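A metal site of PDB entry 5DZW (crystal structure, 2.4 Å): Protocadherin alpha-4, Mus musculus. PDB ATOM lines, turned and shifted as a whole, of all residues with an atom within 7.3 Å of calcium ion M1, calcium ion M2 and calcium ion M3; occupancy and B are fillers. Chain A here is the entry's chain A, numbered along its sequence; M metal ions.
OE1 of Glu 115 lies within hydrogen-bond range of N of Ala 206. OE2 of Glu 115 sits close to N of Arg 173 (3.4 Å). O of Leu 204 sits close to N of Glu 115 (3.4 Å). NE of Arg 173 lies close to OD1 of Asp 205 (3.6 Å). OD2 of Asp 205 is in hydrogen-bond range of N of Glu 242, at 2.9 Å. ND2 of Asn 207 lies within hydrogen-bond range of O of Leu 299 (2.6 Å). N of Leu 301 is in hydrogen-bond range of OD1 of Asp 295 (2.6 Å). The side-chain carboxylate of Asp 172 lies within hydrogen-bond range of the backbone NH of Glu 175 (2.6 Å).
Within 4 Å of calcium ion M1: Asn 207, Asn 209, Asp 239, Asp 241, Asn 245 and Asp 295. The nearest printed residue that does not touch calcium ion M1 is Ala 210 (4.6 Å).
The nearest printed residue that does not touch calcium ion M2 is Arg 173 (4.3 Å).
Five residues have an atom within 4 Å of calcium ion M3: Glu 115, Asp 172, Glu 174, Asp 208 and Asn 209. The nearest printed residue that does not touch calcium ion M3 is Asp 241 (4.1 Å).
Calcium ion M1 is bound by the side-chain carboxylate (OD2) of Asp 239, 2.4 Å away. Calcium ion M1 is bound by O of Asn 209. O of Asn 245 binds calcium ion M1, at 2.6 Å. Calcium ion M1 is bound by the side-chain amide oxygen (OD1) of Asn 207 (2.7 Å). OD2 of Asp 295 binds calcium ion M1 (2.8 Å). The side-chain carboxylate (OD2) of Asp 241 binds calcium ion M1 (2.9 Å). Calcium ion M1 has six donor atoms within binding distance.
Calcium ion M2 is bound by the backbone carbonyl oxygen (O) of Ala 206 (2.4 Å), the side-chain carboxylate (OD1) of Asp 205 (2.5 Å), the side-chain carboxylate (OE2) of Glu 174 (2.5 Å), the side-chain carboxylate (OD1) of Asp 241 (2.6 Å) and the side-chain carboxylate (OD1) of Asp 208 (2.8 Å). Slightly farther from calcium ion M2 lies OE1 of Glu 115 (3.1 Å).
Calcium ion M3 is bound by the side-chain carboxylate (OE1) of Glu 174 (2.4 Å). Calcium ion M3 is bound by the side-chain carboxylate (OE2) of Glu 115, 2.4 Å away. The side-chain carboxylate (OD1) of Asp 208 binds calcium ion M3, at 2.6 Å. Calcium ion M3 is bound by OD2 of Asp 208, at 2.7 Å. Calcium ion M3 has four donor atoms within binding distance. Slightly farther from calcium ion M3 lies the side-chain carboxylate (OD1) of Asp 172 (3.0 Å).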
ATOM      1  N   GLU A 115     -20.077 -28.308   8.672  1.00  0.00           N
ATOM      2  CA  GLU A 115     -18.806 -28.522   9.366  1.00  0.00           C
ATOM      3  C   GLU A 115     -18.344 -27.239  10.062  1.00  0.00           C
ATOM      4  O   GLU A 115     -17.536 -27.283  10.990  1.00  0.00           O
ATOM      5  CB  GLU A 115     -17.747 -28.993   8.369  1.00  0.00           C
ATOM      6  CG  GLU A 115     -16.414 -29.382   8.984  1.00  0.00           C
ATOM      7  CD  GLU A 115     -15.333 -29.593   7.950  1.00  0.00           C
ATOM      8  OE1 GLU A 115     -15.632 -29.497   6.741  1.00  0.00           O
ATOM      9  OE2 GLU A 115     -14.173 -29.845   8.343  1.00  0.00           O
ATOM     10  N   LEU A 171     -16.178 -30.846  14.668  1.00  0.00           N
ATOM     11  CA  LEU A 171     -16.547 -31.804  13.627  1.00  0.00           C
ATOM     12  C   LEU A 171     -15.745 -31.568  12.349  1.00  0.00           C
ATOM     13  O   LEU A 171     -15.522 -30.428  11.943  1.00  0.00           O
ATOM     14  CB  LEU A 171     -18.048 -31.723  13.339  1.00  0.00           C
ATOM     15  CG  LEU A 171     -18.635 -30.532  12.574  1.00  0.00           C
ATOM     16  CD1 LEU A 171     -20.069 -30.825  12.171  1.00  0.00           C
ATOM     17  CD2 LEU A 171     -18.572 -29.235  13.386  1.00  0.00           C
ATOM     18  N   ASP A 172     -15.318 -32.654  11.719  1.00  0.00           N
ATOM     19  CA  ASP A 172     -14.529 -32.580  10.501  1.00  0.00           C
ATOM     20  C   ASP A 172     -15.061 -33.539   9.432  1.00  0.00           C
ATOM     21  O   ASP A 172     -15.070 -34.748   9.631  1.00  0.00           O
ATOM     22  CB  ASP A 172     -13.056 -32.881  10.796  1.00  0.00           C
ATOM     23  CG  ASP A 172     -12.180 -32.792   9.555  1.00  0.00           C
ATOM     24  OD1 ASP A 172     -11.768 -31.661   9.209  1.00  0.00           O
ATOM     25  OD2 ASP A 172     -11.905 -33.837   8.937  1.00  0.00           O
ATOM     26  N   ARG A 173     -15.482 -32.977   8.310  1.00  0.00           N
ATOM     27  CA  ARG A 173     -16.057 -33.740   7.214  1.00  0.00           C
ATOM     28  C   ARG A 173     -15.076 -34.777   6.644  1.00  0.00           C
ATOM     29  O   ARG A 173     -15.476 -35.896   6.319  1.00  0.00           O
ATOM     30  CB  ARG A 173     -16.539 -32.799   6.115  1.00  0.00           C
ATOM     31  CG  ARG A 173     -16.863 -33.459   4.789  1.00  0.00           C
ATOM     32  CD  ARG A 173     -15.814 -33.114   3.737  1.00  0.00           C
ATOM     33  NE  ARG A 173     -16.224 -33.520   2.398  1.00  0.00           N
ATOM     34  CZ  ARG A 173     -15.934 -34.702   1.859  1.00  0.00           C
ATOM     35  NH1 ARG A 173     -16.342 -34.994   0.631  1.00  0.00           N
ATOM     36  NH2 ARG A 173     -15.237 -35.592   2.547  1.00  0.00           N
ATOM     37  N   GLU A 174     -13.814 -34.398   6.527  1.00  0.00           N
ATOM     38  CA  GLU A 174     -12.801 -35.266   5.946  1.00  0.00           C
ATOM     39  C   GLU A 174     -12.494 -36.483   6.817  1.00  0.00           C
ATOM     40  O   GLU A 174     -12.253 -37.571   6.315  1.00  0.00           O
ATOM     41  CB  GLU A 174     -11.507 -34.488   5.668  1.00  0.00           C
ATOM     42  CG  GLU A 174     -11.572 -33.556   4.470  1.00  0.00           C
ATOM     43  CD  GLU A 174     -12.437 -32.335   4.713  1.00  0.00           C
ATOM     44  OE1 GLU A 174     -12.676 -31.999   5.892  1.00  0.00           O
ATOM     45  OE2 GLU A 174     -12.885 -31.716   3.721  1.00  0.00           O
ATOM     46  N   GLU A 175     -12.510 -36.272   8.132  1.00  0.00           N
ATOM     47  CA  GLU A 175     -12.243 -37.362   9.069  1.00  0.00           C
ATOM     48  C   GLU A 175     -13.406 -38.355   9.112  1.00  0.00           C
ATOM     49  O   GLU A 175     -13.215 -39.557   8.905  1.00  0.00           O
ATOM     50  CB  GLU A 175     -11.976 -36.805  10.470  1.00  0.00           C
ATOM     51  CG  GLU A 175     -11.687 -37.864  11.519  1.00  0.00           C
ATOM     52  CD  GLU A 175     -11.276 -37.280  12.853  1.00  0.00           C
ATOM     53  OE1 GLU A 175     -10.761 -36.136  12.861  1.00  0.00           O
ATOM     54  OE2 GLU A 175     -11.459 -37.944  13.888  1.00  0.00           O
ATOM     55  N   LEU A 204     -21.614 -31.489   6.211  1.00  0.00           N
ATOM     56  CA  LEU A 204     -21.397 -30.794   4.954  1.00  0.00           C
ATOM     57  C   LEU A 204     -19.953 -30.311   4.830  1.00  0.00           C
ATOM     58  O   LEU A 204     -19.292 -30.030   5.827  1.00  0.00           O
ATOM     59  CB  LEU A 204     -22.370 -29.621   4.822  1.00  0.00           C
ATOM     60  CG  LEU A 204     -23.842 -29.965   5.044  1.00  0.00           C
ATOM     61  CD1 LEU A 204     -24.730 -28.730   4.949  1.00  0.00           C
ATOM     62  CD2 LEU A 204     -24.302 -31.043   4.067  1.00  0.00           C
ATOM     63  N   ASP A 205     -19.467 -30.228   3.593  1.00  0.00           N
ATOM     64  CA  ASP A 205     -18.073 -29.845   3.349  1.00  0.00           C
ATOM     65  C   ASP A 205     -17.858 -28.338   3.484  1.00  0.00           C
ATOM     66  O   ASP A 205     -18.448 -27.548   2.741  1.00  0.00           O
ATOM     67  CB  ASP A 205     -17.635 -30.312   1.963  1.00  0.00           C
ATOM     68  CG  ASP A 205     -16.186 -29.966   1.662  1.00  0.00           C
ATOM     69  OD1 ASP A 205     -15.356 -30.021   2.588  1.00  0.00           O
ATOM     70  OD2 ASP A 205     -15.880 -29.641   0.496  1.00  0.00           O
ATOM     71  N   ALA A 206     -17.022 -27.952   4.433  1.00  0.00           N
ATOM     72  CA  ALA A 206     -16.647 -26.553   4.611  1.00  0.00           C
ATOM     73  C   ALA A 206     -15.290 -26.295   3.963  1.00  0.00           C
ATOM     74  O   ALA A 206     -14.501 -27.215   3.797  1.00  0.00           O
ATOM     75  CB  ALA A 206     -16.626 -26.189   6.079  1.00  0.00           C
ATOM     76  N   ASN A 207     -15.031 -25.047   3.618  1.00  0.00           N
ATOM     77  CA  ASN A 207     -13.745 -24.685   3.009  1.00  0.00           C
ATOM     78  C   ASN A 207     -12.727 -24.295   4.081  1.00  0.00           C
ATOM     79  O   ASN A 207     -12.342 -23.138   4.197  1.00  0.00           O
ATOM     80  CB  ASN A 207     -13.922 -23.539   2.014  1.00  0.00           C
ATOM     81  CG  ASN A 207     -12.691 -23.325   1.159  1.00  0.00           C
ATOM     82  OD1 ASN A 207     -11.903 -24.240   0.938  1.00  0.00           O
ATOM     83  ND2 ASN A 207     -12.507 -22.091   0.685  1.00  0.00           N
ATOM     84  N   ASP A 208     -12.306 -25.281   4.865  1.00  0.00           N
ATOM     85  CA  ASP A 208     -11.415 -25.029   5.989  1.00  0.00           C
ATOM     86  C   ASP A 208     -10.060 -25.719   5.827  1.00  0.00           C
ATOM     87  O   ASP A 208      -9.281 -25.811   6.777  1.00  0.00           O
ATOM     88  CB  ASP A 208     -12.071 -25.474   7.300  1.00  0.00           C
ATOM     89  CG  ASP A 208     -12.509 -26.925   7.271  1.00  0.00           C
ATOM     90  OD1 ASP A 208     -12.911 -27.404   6.191  1.00  0.00           O
ATOM     91  OD2 ASP A 208     -12.452 -27.580   8.337  1.00  0.00           O
ATOM     92  N   ASN A 209      -9.775 -26.203   4.619  1.00  0.00           N
ATOM     93  CA  ASN A 209      -8.491 -26.814   4.331  1.00  0.00           C
ATOM     94  C   ASN A 209      -7.799 -26.191   3.122  1.00  0.00           C
ATOM     95  O   ASN A 209      -8.383 -26.106   2.038  1.00  0.00           O
ATOM     96  CB  ASN A 209      -8.644 -28.320   4.112  1.00  0.00           C
ATOM     97  CG  ASN A 209      -8.669 -29.103   5.416  1.00  0.00           C
ATOM     98  OD1 ASN A 209      -9.168 -28.614   6.427  1.00  0.00           O
ATOM     99  ND2 ASN A 209      -8.119 -30.309   5.387  1.00  0.00           N
ATOM    100  N   ALA A 210      -6.565 -25.745   3.321  1.00  0.00           N
ATOM    101  CA  ALA A 210      -5.781 -25.131   2.250  1.00  0.00           C
ATOM    102  C   ALA A 210      -5.084 -26.203   1.412  1.00  0.00           C
ATOM    103  O   ALA A 210      -4.749 -27.275   1.916  1.00  0.00           O
ATOM    104  CB  ALA A 210      -4.763 -24.169   2.842  1.00  0.00           C
ATOM    105  N   PRO A 211      -4.862 -25.912   0.115  1.00  0.00           N
ATOM    106  CA  PRO A 211      -4.140 -26.829  -0.757  1.00  0.00           C
ATOM    107  C   PRO A 211      -2.694 -27.034  -0.321  1.00  0.00           C
ATOM    108  O   PRO A 211      -2.103 -26.130   0.276  1.00  0.00           O
ATOM    109  CB  PRO A 211      -4.209 -26.140  -2.126  1.00  0.00           C
ATOM    110  CG  PRO A 211      -4.497 -24.712  -1.833  1.00  0.00           C
ATOM    111  CD  PRO A 211      -5.352 -24.725  -0.603  1.00  0.00           C
ATOM    112  N   ASP A 239      -5.770 -31.049  -2.218  1.00  0.00           N
ATOM    113  CA  ASP A 239      -6.635 -30.411  -1.237  1.00  0.00           C
ATOM    114  C   ASP A 239      -7.742 -31.364  -0.789  1.00  0.00           C
ATOM    115  O   ASP A 239      -8.351 -32.049  -1.609  1.00  0.00           O
ATOM    116  CB  ASP A 239      -7.229 -29.118  -1.811  1.00  0.00           C
ATOM    117  CG  ASP A 239      -7.957 -28.291  -0.768  1.00  0.00           C
ATOM    118  OD1 ASP A 239      -7.780 -28.563   0.445  1.00  0.00           O
ATOM    119  OD2 ASP A 239      -8.695 -27.370  -1.157  1.00  0.00           O
ATOM    120  N   LEU A 240      -7.997 -31.388   0.521  1.00  0.00           N
ATOM    121  CA  LEU A 240      -8.905 -32.370   1.098  1.00  0.00           C
ATOM    122  C   LEU A 240     -10.381 -32.039   0.882  1.00  0.00           C
ATOM    123  O   LEU A 240     -11.228 -32.924   0.927  1.00  0.00           O
ATOM    124  CB  LEU A 240      -8.622 -32.516   2.595  1.00  0.00           C
ATOM    125  CG  LEU A 240      -7.277 -33.142   2.944  1.00  0.00           C
ATOM    126  CD1 LEU A 240      -7.130 -33.320   4.448  1.00  0.00           C
ATOM    127  CD2 LEU A 240      -7.108 -34.482   2.232  1.00  0.00           C
ATOM    128  N   ASP A 241     -10.682 -30.770   0.635  1.00  0.00           N
ATOM    129  CA  ASP A 241     -12.065 -30.362   0.399  1.00  0.00           C
ATOM    130  C   ASP A 241     -12.550 -30.809  -0.974  1.00  0.00           C
ATOM    131  O   ASP A 241     -11.747 -31.191  -1.831  1.00  0.00           O
ATOM    132  CB  ASP A 241     -12.214 -28.845   0.553  1.00  0.00           C
ATOM    133  CG  ASP A 241     -11.840 -28.356   1.932  1.00  0.00           C
ATOM    134  OD1 ASP A 241     -11.550 -29.199   2.805  1.00  0.00           O
ATOM    135  OD2 ASP A 241     -11.853 -27.130   2.156  1.00  0.00           O
ATOM    136  N   GLU A 242     -13.860 -30.765  -1.178  1.00  0.00           N
ATOM    137  CA  GLU A 242     -14.455 -31.234  -2.429  1.00  0.00           C
ATOM    138  C   GLU A 242     -15.170 -30.109  -3.178  1.00  0.00           C
ATOM    139  O   GLU A 242     -15.401 -29.035  -2.628  1.00  0.00           O
ATOM    140  CB  GLU A 242     -15.429 -32.380  -2.153  1.00  0.00           C
ATOM    141  N   VAL A 244     -15.785 -27.039  -5.699  1.00  0.00           N
ATOM    142  CA  VAL A 244     -14.992 -25.874  -6.037  1.00  0.00           C
ATOM    143  C   VAL A 244     -14.009 -25.551  -4.911  1.00  0.00           C
ATOM    144  O   VAL A 244     -13.034 -24.833  -5.108  1.00  0.00           O
ATOM    145  CB  VAL A 244     -15.870 -24.639  -6.317  1.00  0.00           C
ATOM    146  CG1 VAL A 244     -16.733 -24.862  -7.547  1.00  0.00           C
ATOM    147  CG2 VAL A 244     -16.737 -24.305  -5.105  1.00  0.00           C
ATOM    148  N   ASN A 245     -14.282 -26.091  -3.720  1.00  0.00           N
ATOM    149  CA  ASN A 245     -13.389 -25.925  -2.588  1.00  0.00           C
ATOM    150  C   ASN A 245     -12.182 -26.847  -2.693  1.00  0.00           C
ATOM    151  O   ASN A 245     -11.237 -26.736  -1.918  1.00  0.00           O
ATOM    152  CB  ASN A 245     -14.130 -26.182  -1.275  1.00  0.00           C
ATOM    153  CG  ASN A 245     -15.270 -25.202  -1.047  1.00  0.00           C
ATOM    154  OD1 ASN A 245     -15.562 -24.374  -1.901  1.00  0.00           O
ATOM    155  ND2 ASN A 245     -15.909 -25.310   0.104  1.00  0.00           N
ATOM    156  N   GLY A 246     -12.225 -27.745  -3.670  1.00  0.00           N
ATOM    157  CA  GLY A 246     -11.148 -28.696  -3.885  1.00  0.00           C
ATOM    158  C   GLY A 246     -10.298 -28.384  -5.106  1.00  0.00           C
ATOM    159  O   GLY A 246      -9.104 -28.682  -5.139  1.00  0.00           O
ATOM    160  N   ASP A 247     -10.919 -27.785  -6.128  1.00  0.00           N
ATOM    161  CA  ASP A 247     -10.207 -27.437  -7.356  1.00  0.00           C
ATOM    162  C   ASP A 247      -9.185 -26.336  -7.112  1.00  0.00           C
ATOM    163  O   ASP A 247      -9.482 -25.343  -6.454  1.00  0.00           O
ATOM    164  CB  ASP A 247     -11.197 -27.012  -8.444  1.00  0.00           C
ATOM    165  CG  ASP A 247     -11.995 -28.175  -8.999  1.00  0.00           C
ATOM    166  OD1 ASP A 247     -12.315 -29.105  -8.229  1.00  0.00           O
ATOM    167  OD2 ASP A 247     -12.305 -28.162 -10.205  1.00  0.00           O
ATOM    168  N   ILE A 248      -7.976 -26.522  -7.652  1.00  0.00           N
ATOM    169  CA  ILE A 248      -6.875 -25.602  -7.393  1.00  0.00           C
ATOM    170  C   ILE A 248      -6.388 -24.889  -8.653  1.00  0.00           C
ATOM    171  O   ILE A 248      -6.143 -25.516  -9.681  1.00  0.00           O
ATOM    172  CB  ILE A 248      -5.682 -26.348  -6.761  1.00  0.00           C
ATOM    173  CG1 ILE A 248      -6.147 -27.223  -5.592  1.00  0.00           C
ATOM    174  CG2 ILE A 248      -4.612 -25.360  -6.299  1.00  0.00           C
ATOM    175  CD1 ILE A 248      -5.067 -28.113  -5.031  1.00  0.00           C
ATOM    176  N   ASP A 295      -7.518 -22.344  -4.033  1.00  0.00           N
ATOM    177  CA  ASP A 295      -8.757 -23.046  -4.359  1.00  0.00           C
ATOM    178  C   ASP A 295      -9.825 -22.082  -4.848  1.00  0.00           C
ATOM    179  O   ASP A 295      -9.609 -20.872  -4.913  1.00  0.00           O
ATOM    180  CB  ASP A 295      -9.267 -23.848  -3.149  1.00  0.00           C
ATOM    181  CG  ASP A 295      -9.211 -23.060  -1.858  1.00  0.00           C
ATOM    182  OD1 ASP A 295      -9.430 -21.832  -1.892  1.00  0.00           O
ATOM    183  OD2 ASP A 295      -8.955 -23.665  -0.798  1.00  0.00           O
ATOM    184  N   LYS A 296     -10.996 -22.611  -5.200  1.00  0.00           N
ATOM    185  CA  LYS A 296     -12.059 -21.805  -5.793  1.00  0.00           C
ATOM    186  C   LYS A 296     -13.298 -21.736  -4.911  1.00  0.00           C
ATOM    187  O   LYS A 296     -14.422 -21.820  -5.405  1.00  0.00           O
ATOM    188  CB  LYS A 296     -12.426 -22.366  -7.174  1.00  0.00           C
ATOM    189  CG  LYS A 296     -11.257 -22.496  -8.133  1.00  0.00           C
ATOM    190  CD  LYS A 296     -11.691 -23.114  -9.454  1.00  0.00           C
ATOM    191  N   GLY A 297     -13.095 -21.577  -3.607  1.00  0.00           N
ATOM    192  CA  GLY A 297     -14.196 -21.472  -2.674  1.00  0.00           C
ATOM    193  C   GLY A 297     -14.649 -20.043  -2.489  1.00  0.00           C
ATOM    194  O   GLY A 297     -14.075 -19.118  -3.069  1.00  0.00           O
ATOM    195  N   LEU A 299     -14.526 -18.307   0.372  1.00  0.00           N
ATOM    196  CA  LEU A 299     -13.361 -17.740   1.032  1.00  0.00           C
ATOM    197  C   LEU A 299     -12.143 -18.568   0.666  1.00  0.00           C
ATOM    198  O   LEU A 299     -11.881 -19.601   1.293  1.00  0.00           O
ATOM    199  CB  LEU A 299     -13.548 -17.688   2.549  1.00  0.00           C
ATOM    200  CG  LEU A 299     -12.388 -17.085   3.336  1.00  0.00           C
ATOM    201  CD1 LEU A 299     -12.054 -15.695   2.816  1.00  0.00           C
ATOM    202  CD2 LEU A 299     -12.695 -17.053   4.820  1.00  0.00           C
ATOM    203  N   PRO A 300     -11.398 -18.133  -0.360  1.00  0.00           N
ATOM    204  CA  PRO A 300     -10.266 -18.885  -0.915  1.00  0.00           C
ATOM    205  C   PRO A 300      -9.140 -19.109   0.079  1.00  0.00           C
ATOM    206  O   PRO A 300      -8.795 -18.197   0.845  1.00  0.00           O
ATOM    207  CB  PRO A 300      -9.798 -18.003  -2.072  1.00  0.00           C
ATOM    208  CG  PRO A 300     -10.966 -17.134  -2.408  1.00  0.00           C
ATOM    209  CD  PRO A 300     -11.643 -16.881  -1.101  1.00  0.00           C
ATOM    210  N   LEU A 301      -8.573 -20.308   0.067  1.00  0.00           N
ATOM    211  CA  LEU A 301      -7.375 -20.608   0.849  1.00  0.00           C
ATOM    212  C   LEU A 301      -6.197 -20.857  -0.092  1.00  0.00           C
ATOM    213  O   LEU A 301      -6.364 -21.421  -1.178  1.00  0.00           O
ATOM    214  CB  LEU A 301      -7.603 -21.824   1.745  1.00  0.00           C
ATOM    215  CG  LEU A 301      -8.587 -21.628   2.901  1.00  0.00           C
ATOM    216  CD1 LEU A 301      -8.618 -22.858   3.795  1.00  0.00           C
ATOM    217  CD2 LEU A 301      -8.230 -20.384   3.701  1.00  0.00           C
HETATM  218 CA    CA M   1     -10.031 -26.000   0.235  1.00  0.00          CA
HETATM  219 CA    CA M   2     -13.700 -29.386   4.306  1.00  0.00          CA
HETATM  220 CA    CA M   3     -12.246 -29.801   6.843  1.00  0.00          CA
